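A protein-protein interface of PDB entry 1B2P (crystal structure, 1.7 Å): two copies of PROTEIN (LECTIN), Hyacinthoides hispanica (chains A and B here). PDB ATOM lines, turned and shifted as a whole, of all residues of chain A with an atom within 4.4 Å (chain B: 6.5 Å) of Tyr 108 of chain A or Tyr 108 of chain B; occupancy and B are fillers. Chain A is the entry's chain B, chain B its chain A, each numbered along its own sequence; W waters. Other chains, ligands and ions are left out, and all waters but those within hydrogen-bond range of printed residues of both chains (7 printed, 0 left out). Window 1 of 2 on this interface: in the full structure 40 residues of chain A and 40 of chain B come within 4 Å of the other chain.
Val 106 of chain A touches Ala 111 of chain B, and with the chains exchanged Ala 111 of chain A touches Val 106 of chain B. Ile 107 of chain A touches Ala 111 of chain B, and with the chains exchanged Ala 111 of chain A touches Ile 107 of chain B. Tyr 108 of chain A touches Ala 111 of chain B, and with the chains exchanged Ala 111 of chain A touches Tyr 108 of chain B. Gly 109 of chain B touches its own counterpart, Gly 109 of chain A. Positions printed for both chains: 94, 95, 96, 98, 100, 106, 107, 108, 109, 110 and 111.
Hydrophobic or aromatic side chains of chain A within 4 Å of the printed part of chain B: His 94, Tyr 95, Val 96, Val 98, Val 106, Ile 107, Tyr 108 and Ala 111. Among the printed residues, no Asp or Glu carboxylate lies within 4 Å of a Lys or Arg side-chain nitrogen of the other chain.
The side-chain hydroxyl of Ser 6 of chain B sits at hydrogen-bond distance from the backbone NH of Tyr 95 of chain B (2.9 Å). The side-chain amide oxygen (OE1) of Gln 8 of chain B lies close to the side-chain amide oxygen (OD1) of Asn 12 of chain B. The side-chain hydroxyl of Tyr 108 of chain B is in hydrogen-bond range of the side-chain amide oxygen of Gln 100 of chain B (2.6 Å). The side-chain carboxylate of Asp 110 of chain A lies within hydrogen-bond range of the backbone NH of His 94 of chain A (2.9 Å). The backbone NH (N) of Ala 111 of chain A lies within hydrogen-bond range of the backbone carbonyl oxygen (O) of His 94 of chain A. The backbone carbonyl oxygen (O) of Val 96 of chain A sits at hydrogen-bond distance from the backbone NH (N) of Tyr 108 of chain A, 2.8 Å away.
Water W6 lies within hydrogen-bond range of OE1 of Gln 8 of chain B, ND1 of His 94 of chain B, OD1 of Asn 12 of chain B, NE2 of Gln 100 of chain A and OH of Tyr 108 of chain A. Water W1 lies within hydrogen-bond range of a ring nitrogen (ND1) of His 94 of chain B (2.7 Å) and the side-chain hydroxyl (OH) of Tyr 108 of chain A (3.2 Å). Water W4 bridges O of Tyr 95 of chain A (2.8 Å) and OH of Tyr 108 of chain B (2.9 Å). Water W3 lies within hydrogen-bond range of O of Gly 109 of chain A and O of Asp 110 of chain B. Water W7 lies within hydrogen-bond range of the side-chain hydroxyl of Tyr 108 of chain A (2.9 Å), the backbone carbonyl oxygen of Tyr 95 of chain B (2.9 Å) and the side-chain amide nitrogen of Gln 8 of chain B (2.9 Å). Water W5 lies within hydrogen-bond range of the backbone carbonyl oxygen of Gly 109 of chain B (3.1 Å), the backbone NH of Asp 110 of chain B (3.4 Å) and the backbone carbonyl oxygen of Gly 109 of chain A (3.5 Å).
The side-chain amide oxygen (OD1) of Asn 12 of chain B lies within hydrogen-bond range of the side-chain amide nitrogen (NE2) of Gln 100 of chain A (3.3 Å). The backbone NH (N) of Gly 109 of chain B is in hydrogen-bond range of the backbone carbonyl oxygen (O) of Asp 110 of chain A. O of Asp 110 of chain B lies within hydrogen-bond range of N of Gly 109 of chain A (3.4 Å). N of Leu 112 of chain B is in hydrogen-bond range of O of Ile 107 of chain A (2.8 Å). N of Ile 107 of chain A sits at hydrogen-bond distance from O of Trp 113 of chain B (2.8 Å). O of Gly 109 of chain B sits close to O of Gly 109 of chain A (3.5 Å).
Printed residues of chain B within 4 Å of Tyr 108 of chain A: His 94 (3.4 Å), Tyr 95 (3.99 Å), Val 96 (3.6 Å), Tyr 108 (3.8 Å), Asp 110 (3.9 Å) and Ala 111 (3.9 Å). Of the printed residues of chain A, Tyr 108 of chain B touches His 94 (3.5 Å), Val 96 (3.6 Å), Tyr 108 (3.8 Å), Asp 110 (3.8 Å) and Ala 111 (3.8 Å). Of the printed residues of chain A, Ile 3 of chain B touches Val 98. Printed residues of chain B within 4 Å of Tyr 95 of chain A: Leu 112. Leu 97 of chain B touches none of the printed residues of chain A. The nearest residue of chain A that does not touch Tyr 108 of chain B is Tyr 95 of chain A (4.04 Å). The nearest printed residue of chain B that does not touch Asp 110 of chain A is Ile 107 of chain B (4.4 Å).
Among the printed residues, pairs that only touch across the chains: His 94 of chain A with Tyr 108 of chain B (3.5 Å), Tyr 95 of chain A with Leu 112 of chain B (3.9 Å), Val 96 of chain A with Tyr 108 of chain B (3.6 Å), Val 98 of chain A with Ile 3 of chain B (3.8 Å), Gln 100 of chain A with Phe 5 of chain B (3.7 Å), Val 106 of chain A with Ala 111 of chain B (3.6 Å), Val 106 of chain A with Trp 113 of chain B (3.5 Å), Ile 107 of chain A with Ala 111 of chain B (3.6 Å), Tyr 108 of chain A with His 94 of chain B (3.4 Å), Tyr 108 of chain A with Tyr 95 of chain B (3.99 Å), Tyr 108 of chain A with Val 96 of chain B (3.6 Å), Tyr 108 of chain A with Tyr 108 of chain B (3.8 Å), Tyr 108 of chain A with Asp 110 of chain B (3.9 Å), Tyr 108 of chain A with Ala 111 of chain B (3.9 Å), Asp 110 of chain A with Tyr 108 of chain B (3.8 Å), Ala 111 of chain A with Val 106 of chain B (3.6 Å), Ala 111 of chain A with Ile 107 of chain B (3.6 Å) and Ala 111 of chain A with Tyr 108 of chain B (3.8 Å).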
ATOM      1  N   HIS A  94      17.639  -3.592  -9.815  1.00  0.00           N
ATOM      2  CA  HIS A  94      16.899  -3.673  -8.563  1.00  0.00           C
ATOM      3  C   HIS A  94      17.916  -3.379  -7.433  1.00  0.00           C
ATOM      4  O   HIS A  94      19.018  -3.860  -7.581  1.00  0.00           O
ATOM      5  CB  HIS A  94      16.450  -5.150  -8.345  1.00  0.00           C
ATOM      6  CG  HIS A  94      15.404  -5.521  -9.414  1.00  0.00           C
ATOM      7  ND1 HIS A  94      15.814  -6.040 -10.620  1.00  0.00           N
ATOM      8  CD2 HIS A  94      14.071  -5.449  -9.291  1.00  0.00           C
ATOM      9  CE1 HIS A  94      14.674  -6.283 -11.278  1.00  0.00           C
ATOM     10  NE2 HIS A  94      13.601  -5.973 -10.521  1.00  0.00           N
ATOM     11  N   TYR A  95      17.443  -2.587  -6.497  1.00  0.00           N
ATOM     12  CA  TYR A  95      18.394  -2.206  -5.402  1.00  0.00           C
ATOM     13  C   TYR A  95      17.545  -2.358  -4.167  1.00  0.00           C
ATOM     14  O   TYR A  95      16.325  -2.434  -4.066  1.00  0.00           O
ATOM     15  CB  TYR A  95      18.762  -0.672  -5.532  1.00  0.00           C
ATOM     16  CG  TYR A  95      19.727  -0.479  -6.673  1.00  0.00           C
ATOM     17  CD1 TYR A  95      19.271  -0.448  -8.034  1.00  0.00           C
ATOM     18  CD2 TYR A  95      21.079  -0.333  -6.429  1.00  0.00           C
ATOM     19  CE1 TYR A  95      20.195  -0.289  -9.086  1.00  0.00           C
ATOM     20  CE2 TYR A  95      22.005  -0.203  -7.461  1.00  0.00           C
ATOM     21  CZ  TYR A  95      21.523  -0.153  -8.753  1.00  0.00           C
ATOM     22  OH  TYR A  95      22.382  -0.041  -9.850  1.00  0.00           O
ATOM     23  N   VAL A  96      18.344  -2.430  -3.014  1.00  0.00           N
ATOM     24  CA  VAL A  96      17.703  -2.300  -1.740  1.00  0.00           C
ATOM     25  C   VAL A  96      18.448  -1.253  -0.803  1.00  0.00           C
ATOM     26  O   VAL A  96      19.658  -1.142  -0.987  1.00  0.00           O
ATOM     27  CB  VAL A  96      17.681  -3.628  -0.907  1.00  0.00           C
ATOM     28  CG1 VAL A  96      16.765  -4.670  -1.674  1.00  0.00           C
ATOM     29  CG2 VAL A  96      19.073  -4.262  -0.800  1.00  0.00           C
ATOM     30  N   VAL A  98      19.247  -0.619   3.177  1.00  0.00           N
ATOM     31  CA  VAL A  98      19.101  -1.387   4.433  1.00  0.00           C
ATOM     32  C   VAL A  98      19.534  -0.521   5.652  1.00  0.00           C
ATOM     33  O   VAL A  98      20.627   0.036   5.473  1.00  0.00           O
ATOM     34  CB  VAL A  98      20.022  -2.601   4.348  1.00  0.00           C
ATOM     35  CG1 VAL A  98      19.846  -3.511   5.585  1.00  0.00           C
ATOM     36  CG2 VAL A  98      19.682  -3.433   3.051  1.00  0.00           C
ATOM     37  N   GLN A 100      21.147  -0.896   8.950  1.00  0.00           N
ATOM     38  CA  GLN A 100      21.949  -2.099   9.407  1.00  0.00           C
ATOM     39  C   GLN A 100      22.269  -2.024  10.894  1.00  0.00           C
ATOM     40  O   GLN A 100      22.191  -1.007  11.529  1.00  0.00           O
ATOM     41  CB  GLN A 100      23.325  -2.039   8.730  1.00  0.00           C
ATOM     42  CG  GLN A 100      23.120  -2.163   7.216  1.00  0.00           C
ATOM     43  CD  GLN A 100      24.377  -2.234   6.453  1.00  0.00           C
ATOM     44  OE1 GLN A 100      24.423  -2.724   5.298  1.00  0.00           O
ATOM     45  NE2 GLN A 100      25.594  -1.781   6.939  1.00  0.00           N
ATOM     46  N   VAL A 106      22.651   1.703   4.001  1.00  0.00           N
ATOM     47  CA  VAL A 106      23.459   1.422   2.785  1.00  0.00           C
ATOM     48  C   VAL A 106      22.534   0.986   1.638  1.00  0.00           C
ATOM     49  O   VAL A 106      21.555   0.315   1.915  1.00  0.00           O
ATOM     50  CB  VAL A 106      24.495   0.303   3.025  1.00  0.00           C
ATOM     51  CG1 VAL A 106      25.419   0.095   1.853  1.00  0.00           C
ATOM     52  CG2 VAL A 106      25.333   0.607   4.311  1.00  0.00           C
ATOM     53  N   ILE A 107      22.839   1.517   0.436  1.00  0.00           N
ATOM     54  CA  ILE A 107      22.045   0.996  -0.716  1.00  0.00           C
ATOM     55  C   ILE A 107      22.952   0.002  -1.435  1.00  0.00           C
ATOM     56  O   ILE A 107      24.073   0.314  -1.767  1.00  0.00           O
ATOM     57  CB  ILE A 107      21.772   2.250  -1.624  1.00  0.00           C
ATOM     58  CG1 ILE A 107      20.861   3.223  -0.892  1.00  0.00           C
ATOM     59  CG2 ILE A 107      21.135   1.702  -2.969  1.00  0.00           C
ATOM     60  CD1 ILE A 107      20.747   4.560  -1.698  1.00  0.00           C
ATOM     61  N   TYR A 108      22.390  -1.209  -1.656  1.00  0.00           N
ATOM     62  CA  TYR A 108      23.128  -2.211  -2.351  1.00  0.00           C
ATOM     63  C   TYR A 108      22.377  -2.535  -3.719  1.00  0.00           C
ATOM     64  O   TYR A 108      21.174  -2.609  -3.741  1.00  0.00           O
ATOM     65  CB  TYR A 108      23.028  -3.544  -1.528  1.00  0.00           C
ATOM     66  CG  TYR A 108      23.814  -3.525  -0.195  1.00  0.00           C
ATOM     67  CD1 TYR A 108      25.161  -3.882  -0.240  1.00  0.00           C
ATOM     68  CD2 TYR A 108      23.116  -3.196   0.973  1.00  0.00           C
ATOM     69  CE1 TYR A 108      25.814  -3.869   1.001  1.00  0.00           C
ATOM     70  CE2 TYR A 108      23.802  -3.138   2.219  1.00  0.00           C
ATOM     71  CZ  TYR A 108      25.121  -3.518   2.150  1.00  0.00           C
ATOM     72  OH  TYR A 108      25.852  -3.462   3.357  1.00  0.00           O
ATOM     73  N   GLY A 109      23.245  -2.789  -4.690  1.00  0.00           N
ATOM     74  CA  GLY A 109      22.600  -3.405  -5.905  1.00  0.00           C
ATOM     75  C   GLY A 109      23.668  -3.175  -6.949  1.00  0.00           C
ATOM     76  O   GLY A 109      24.727  -2.572  -6.849  1.00  0.00           O
ATOM     77  N   ASP A 110      23.371  -3.494  -8.269  1.00  0.00           N
ATOM     78  CA  ASP A 110      22.160  -4.218  -8.619  1.00  0.00           C
ATOM     79  C   ASP A 110      22.254  -5.648  -8.181  1.00  0.00           C
ATOM     80  O   ASP A 110      23.172  -6.173  -7.519  1.00  0.00           O
ATOM     81  CB  ASP A 110      22.368  -4.195 -10.209  1.00  0.00           C
ATOM     82  CG  ASP A 110      21.221  -4.728 -11.009  1.00  0.00           C
ATOM     83  OD1 ASP A 110      20.107  -4.889 -10.557  1.00  0.00           O
ATOM     84  OD2 ASP A 110      21.562  -5.026 -12.253  1.00  0.00           O
ATOM     85  N   ALA A 111      21.150  -6.330  -8.400  1.00  0.00           N
ATOM     86  CA  ALA A 111      21.016  -7.737  -8.003  1.00  0.00           C
ATOM     87  C   ALA A 111      22.039  -8.571  -8.710  1.00  0.00           C
ATOM     88  O   ALA A 111      22.193  -8.535  -9.956  1.00  0.00           O
ATOM     89  CB  ALA A 111      19.600  -8.272  -8.310  1.00  0.00           C
ATOM     90  N   ILE B   3      17.800 -11.175   6.360  1.00  0.00           N
ATOM     91  CA  ILE B   3      18.995 -10.761   5.632  1.00  0.00           C
ATOM     92  C   ILE B   3      20.279 -11.440   6.133  1.00  0.00           C
ATOM     93  O   ILE B   3      20.332 -11.735   7.356  1.00  0.00           O
ATOM     94  CB  ILE B   3      19.170  -9.213   5.743  1.00  0.00           C
ATOM     95  CG1 ILE B   3      20.448  -8.709   5.091  1.00  0.00           C
ATOM     96  CG2 ILE B   3      19.247  -8.842   7.258  1.00  0.00           C
ATOM     97  CD1 ILE B   3      20.315  -7.199   4.707  1.00  0.00           C
ATOM     98  N   PHE B   5      24.347 -10.771   5.973  1.00  0.00           N
ATOM     99  CA  PHE B   5      25.417  -9.915   5.482  1.00  0.00           C
ATOM    100  C   PHE B   5      26.699 -10.614   5.123  1.00  0.00           C
ATOM    101  O   PHE B   5      26.963 -11.698   5.675  1.00  0.00           O
ATOM    102  CB  PHE B   5      25.754  -8.933   6.613  1.00  0.00           C
ATOM    103  CG  PHE B   5      24.609  -8.079   7.051  1.00  0.00           C
ATOM    104  CD1 PHE B   5      24.538  -6.837   6.320  1.00  0.00           C
ATOM    105  CD2 PHE B   5      23.705  -8.320   8.042  1.00  0.00           C
ATOM    106  CE1 PHE B   5      23.458  -6.016   6.701  1.00  0.00           C
ATOM    107  CE2 PHE B   5      22.633  -7.513   8.372  1.00  0.00           C
ATOM    108  CZ  PHE B   5      22.536  -6.292   7.710  1.00  0.00           C
ATOM    109  N   SER B   6      27.354 -10.163   4.075  1.00  0.00           N
ATOM    110  CA  SER B   6      28.574 -10.757   3.610  1.00  0.00           C
ATOM    111  C   SER B   6      29.633 -10.693   4.786  1.00  0.00           C
ATOM    112  O   SER B   6      29.537  -9.828   5.568  1.00  0.00           O
ATOM    113  CB  SER B   6      29.154 -10.196   2.315  1.00  0.00           C
ATOM    114  OG  SER B   6      29.404  -8.771   2.511  1.00  0.00           O
ATOM    115  N   GLN B   8      32.286  -9.738   7.001  1.00  0.00           N
ATOM    116  CA  GLN B   8      33.026  -8.445   7.052  1.00  0.00           C
ATOM    117  C   GLN B   8      33.284  -8.114   8.522  1.00  0.00           C
ATOM    118  O   GLN B   8      32.703  -8.598   9.443  1.00  0.00           O
ATOM    119  CB  GLN B   8      32.003  -7.383   6.468  1.00  0.00           C
ATOM    120  CG  GLN B   8      30.680  -7.367   7.207  1.00  0.00           C
ATOM    121  CD  GLN B   8      29.691  -6.427   6.474  1.00  0.00           C
ATOM    122  OE1 GLN B   8      29.507  -5.211   6.744  1.00  0.00           O
ATOM    123  NE2 GLN B   8      28.957  -7.093   5.576  1.00  0.00           N
ATOM    124  N   ASN B  12      27.661  -6.291  11.736  1.00  0.00           N
ATOM    125  CA  ASN B  12      26.380  -6.606  11.065  1.00  0.00           C
ATOM    126  C   ASN B  12      26.251  -8.159  11.262  1.00  0.00           C
ATOM    127  O   ASN B  12      27.267  -8.812  11.049  1.00  0.00           O
ATOM    128  CB  ASN B  12      26.559  -6.254   9.612  1.00  0.00           C
ATOM    129  CG  ASN B  12      26.532  -4.743   9.326  1.00  0.00           C
ATOM    130  OD1 ASN B  12      27.214  -4.319   8.364  1.00  0.00           O
ATOM    131  ND2 ASN B  12      25.776  -4.115  10.106  1.00  0.00           N
ATOM    132  N   LEU B  67      28.011 -15.842   3.106  1.00  0.00           N
ATOM    133  CA  LEU B  67      28.047 -15.016   1.913  1.00  0.00           C
ATOM    134  C   LEU B  67      29.408 -14.375   1.822  1.00  0.00           C
ATOM    135  O   LEU B  67      29.814 -13.710   2.768  1.00  0.00           O
ATOM    136  CB  LEU B  67      26.893 -13.971   2.058  1.00  0.00           C
ATOM    137  CG  LEU B  67      26.850 -13.115   0.804  1.00  0.00           C
ATOM    138  CD1 LEU B  67      26.465 -13.806  -0.520  1.00  0.00           C
ATOM    139  CD2 LEU B  67      25.766 -12.033   1.071  1.00  0.00           C
ATOM    140  N   HIS B  94      30.953  -5.304  -0.088  1.00  0.00           N
ATOM    141  CA  HIS B  94      29.967  -5.684   0.862  1.00  0.00           C
ATOM    142  C   HIS B  94      28.660  -6.065   0.094  1.00  0.00           C
ATOM    143  O   HIS B  94      28.348  -5.286  -0.784  1.00  0.00           O
ATOM    144  CB  HIS B  94      29.536  -4.587   1.814  1.00  0.00           C
ATOM    145  CG  HIS B  94      30.696  -4.303   2.763  1.00  0.00           C
ATOM    146  ND1 HIS B  94      30.498  -3.332   3.773  1.00  0.00           N
ATOM    147  CD2 HIS B  94      31.799  -4.976   3.075  1.00  0.00           C
ATOM    148  CE1 HIS B  94      31.668  -3.364   4.523  1.00  0.00           C
ATOM    149  NE2 HIS B  94      32.444  -4.248   4.090  1.00  0.00           N
ATOM    150  N   TYR B  95      28.070  -7.129   0.518  1.00  0.00           N
ATOM    151  CA  TYR B  95      26.866  -7.605  -0.247  1.00  0.00           C
ATOM    152  C   TYR B  95      25.867  -8.048   0.823  1.00  0.00           C
ATOM    153  O   TYR B  95      26.166  -8.296   2.019  1.00  0.00           O
ATOM    154  CB  TYR B  95      27.216  -8.929  -1.002  1.00  0.00           C
ATOM    155  CG  TYR B  95      28.086  -8.611  -2.177  1.00  0.00           C
ATOM    156  CD1 TYR B  95      29.470  -8.421  -2.108  1.00  0.00           C
ATOM    157  CD2 TYR B  95      27.454  -8.548  -3.502  1.00  0.00           C
ATOM    158  CE1 TYR B  95      30.261  -8.119  -3.205  1.00  0.00           C
ATOM    159  CE2 TYR B  95      28.286  -8.225  -4.553  1.00  0.00           C
ATOM    160  CZ  TYR B  95      29.650  -7.996  -4.438  1.00  0.00           C
ATOM    161  OH  TYR B  95      30.447  -7.652  -5.527  1.00  0.00           O
ATOM    162  N   VAL B  96      24.599  -8.193   0.441  1.00  0.00           N
ATOM    163  CA  VAL B  96      23.553  -8.757   1.297  1.00  0.00           C
ATOM    164  C   VAL B  96      22.645  -9.756   0.488  1.00  0.00           C
ATOM    165  O   VAL B  96      22.602  -9.685  -0.730  1.00  0.00           O
ATOM    166  CB  VAL B  96      22.536  -7.703   1.867  1.00  0.00           C
ATOM    167  CG1 VAL B  96      23.259  -6.688   2.806  1.00  0.00           C
ATOM    168  CG2 VAL B  96      21.953  -6.854   0.694  1.00  0.00           C
ATOM    169  N   LEU B  97      22.283 -10.775   1.240  1.00  0.00           N
ATOM    170  CA  LEU B  97      21.285 -11.719   0.688  1.00  0.00           C
ATOM    171  C   LEU B  97      19.996 -11.466   1.384  1.00  0.00           C
ATOM    172  O   LEU B  97      19.884 -11.358   2.597  1.00  0.00           O
ATOM    173  CB  LEU B  97      21.819 -13.166   0.911  1.00  0.00           C
ATOM    174  CG  LEU B  97      20.763 -14.245   0.531  1.00  0.00           C
ATOM    175  CD1 LEU B  97      21.566 -15.553   0.198  1.00  0.00           C
ATOM    176  CD2 LEU B  97      19.824 -14.519   1.709  1.00  0.00           C
ATOM    177  N   VAL B  98      18.856 -11.309   0.619  1.00  0.00           N
ATOM    178  CA  VAL B  98      17.608 -10.974   1.270  1.00  0.00           C
ATOM    179  C   VAL B  98      16.506 -12.006   0.894  1.00  0.00           C
ATOM    180  O   VAL B  98      16.442 -12.265  -0.323  1.00  0.00           O
ATOM    181  CB  VAL B  98      17.101  -9.585   0.714  1.00  0.00           C
ATOM    182  CG1 VAL B  98      15.840  -9.137   1.423  1.00  0.00           C
ATOM    183  CG2 VAL B  98      18.267  -8.535   0.856  1.00  0.00           C
ATOM    184  N   GLN B 100      12.870 -12.132   0.324  1.00  0.00           N
ATOM    185  CA  GLN B 100      11.943 -10.960   0.021  1.00  0.00           C
ATOM    186  C   GLN B 100      10.513 -11.336   0.092  1.00  0.00           C
ATOM    187  O   GLN B 100      10.134 -12.525  -0.030  1.00  0.00           O
ATOM    188  CB  GLN B 100      12.160 -10.604  -1.455  1.00  0.00           C
ATOM    189  CG  GLN B 100      13.662 -10.192  -1.650  1.00  0.00           C
ATOM    190  CD  GLN B 100      13.951  -9.583  -2.958  1.00  0.00           C
ATOM    191  OE1 GLN B 100      14.967  -8.877  -3.114  1.00  0.00           O
ATOM    192  NE2 GLN B 100      13.223  -9.837  -4.079  1.00  0.00           N
ATOM    193  N   VAL B 106      17.563 -13.026  -3.086  1.00  0.00           N
ATOM    194  CA  VAL B 106      18.352 -12.273  -3.967  1.00  0.00           C
ATOM    195  C   VAL B 106      19.663 -11.788  -3.233  1.00  0.00           C
ATOM    196  O   VAL B 106      19.474 -11.361  -2.121  1.00  0.00           O
ATOM    197  CB  VAL B 106      17.558 -11.036  -4.516  1.00  0.00           C
ATOM    198  CG1 VAL B 106      18.301 -10.323  -5.620  1.00  0.00           C
ATOM    199  CG2 VAL B 106      16.130 -11.436  -5.024  1.00  0.00           C
ATOM    200  N   ILE B 107      20.711 -11.850  -4.015  1.00  0.00           N
ATOM    201  CA  ILE B 107      21.955 -11.276  -3.455  1.00  0.00           C
ATOM    202  C   ILE B 107      22.129  -9.912  -4.111  1.00  0.00           C
ATOM    203  O   ILE B 107      22.156  -9.862  -5.345  1.00  0.00           O
ATOM    204  CB  ILE B 107      23.159 -12.168  -3.812  1.00  0.00           C
ATOM    205  CG1 ILE B 107      22.930 -13.496  -3.097  1.00  0.00           C
ATOM    206  CG2 ILE B 107      24.486 -11.467  -3.377  1.00  0.00           C
ATOM    207  CD1 ILE B 107      24.094 -14.571  -3.453  1.00  0.00           C
ATOM    208  N   TYR B 108      22.334  -8.838  -3.397  1.00  0.00           N
ATOM    209  CA  TYR B 108      22.621  -7.551  -3.976  1.00  0.00           C
ATOM    210  C   TYR B 108      24.028  -7.030  -3.544  1.00  0.00           C
ATOM    211  O   TYR B 108      24.331  -7.248  -2.390  1.00  0.00           O
ATOM    212  CB  TYR B 108      21.587  -6.523  -3.335  1.00  0.00           C
ATOM    213  CG  TYR B 108      20.129  -6.753  -3.672  1.00  0.00           C
ATOM    214  CD1 TYR B 108      19.649  -6.126  -4.820  1.00  0.00           C
ATOM    215  CD2 TYR B 108      19.308  -7.543  -2.888  1.00  0.00           C
ATOM    216  CE1 TYR B 108      18.304  -6.307  -5.176  1.00  0.00           C
ATOM    217  CE2 TYR B 108      17.934  -7.714  -3.204  1.00  0.00           C
ATOM    218  CZ  TYR B 108      17.520  -7.086  -4.380  1.00  0.00           C
ATOM    219  OH  TYR B 108      16.175  -7.265  -4.691  1.00  0.00           O
ATOM    220  N   GLY B 109      24.618  -6.309  -4.486  1.00  0.00           N
ATOM    221  CA  GLY B 109      25.839  -5.547  -3.985  1.00  0.00           C
ATOM    222  C   GLY B 109      26.551  -5.285  -5.252  1.00  0.00           C
ATOM    223  O   GLY B 109      26.220  -5.661  -6.391  1.00  0.00           O
ATOM    224  N   ASP B 110      27.732  -4.649  -5.172  1.00  0.00           N
ATOM    225  CA  ASP B 110      28.221  -4.195  -3.862  1.00  0.00           C
ATOM    226  C   ASP B 110      27.601  -2.921  -3.453  1.00  0.00           C
ATOM    227  O   ASP B 110      26.605  -2.461  -4.032  1.00  0.00           O
ATOM    228  CB  ASP B 110      29.766  -4.089  -3.980  1.00  0.00           C
ATOM    229  CG  ASP B 110      30.380  -2.938  -4.624  1.00  0.00           C
ATOM    230  OD1 ASP B 110      29.717  -2.268  -5.403  1.00  0.00           O
ATOM    231  OD2 ASP B 110      31.614  -2.750  -4.350  1.00  0.00           O
ATOM    232  N   ALA B 111      28.012  -2.280  -2.361  1.00  0.00           N
ATOM    233  CA  ALA B 111      27.344  -1.075  -1.859  1.00  0.00           C
ATOM    234  C   ALA B 111      27.552   0.082  -2.782  1.00  0.00           C
ATOM    235  O   ALA B 111      28.686   0.426  -3.287  1.00  0.00           O
ATOM    236  CB  ALA B 111      28.002  -0.671  -0.503  1.00  0.00           C
ATOM    237  N   LEU B 112      26.447   0.762  -3.115  1.00  0.00           N
ATOM    238  CA  LEU B 112      26.526   1.893  -4.028  1.00  0.00           C
ATOM    239  C   LEU B 112      26.701   3.170  -3.255  1.00  0.00           C
ATOM    240  O   LEU B 112      27.559   3.974  -3.788  1.00  0.00           O
ATOM    241  CB  LEU B 112      25.121   1.944  -4.769  1.00  0.00           C
ATOM    242  CG  LEU B 112      25.047   3.126  -5.776  1.00  0.00           C
ATOM    243  CD1 LEU B 112      25.910   2.775  -7.004  1.00  0.00           C
ATOM    244  CD2 LEU B 112      23.541   3.124  -6.240  1.00  0.00           C
ATOM    245  N   TRP B 113      26.084   3.397  -2.149  1.00  0.00           N
ATOM    246  CA  TRP B 113      26.181   4.599  -1.353  1.00  0.00           C
ATOM    247  C   TRP B 113      25.759   4.305   0.062  1.00  0.00           C
ATOM    248  O   TRP B 113      24.949   3.355   0.315  1.00  0.00           O
ATOM    249  CB  TRP B 113      25.180   5.668  -1.963  1.00  0.00           C
ATOM    250  CG  TRP B 113      25.108   6.934  -1.160  1.00  0.00           C
ATOM    251  CD1 TRP B 113      26.048   7.957  -1.290  1.00  0.00           C
ATOM    252  CD2 TRP B 113      24.128   7.283  -0.200  1.00  0.00           C
ATOM    253  NE1 TRP B 113      25.624   8.917  -0.395  1.00  0.00           N
ATOM    254  CE2 TRP B 113      24.486   8.593   0.264  1.00  0.00           C
ATOM    255  CE3 TRP B 113      23.023   6.663   0.339  1.00  0.00           C
ATOM    256  CZ2 TRP B 113      23.727   9.192   1.245  1.00  0.00           C
ATOM    257  CZ3 TRP B 113      22.240   7.294   1.279  1.00  0.00           C
ATOM    258  CH2 TRP B 113      22.625   8.565   1.726  1.00  0.00           C
HETATM  259  O   HOH W   1      28.449  -1.650   3.393  1.00  0.00           O
HETATM  260  O   HOH W   2      25.636  -6.087  -8.949  1.00  0.00           O
HETATM  261  O   HOH W   3      27.089  -1.018  -6.503  1.00  0.00           O
HETATM  262  O   HOH W   4      14.989  -4.690  -5.114  1.00  0.00           O
HETATM  263  O   HOH W   5      27.517  -3.827  -8.461  1.00  0.00           O
HETATM  264  O   HOH W   6      28.325  -3.205   5.710  1.00  0.00           O
HETATM  265  O   HOH W   7      26.982  -6.064   3.692  1.00  0.00           O
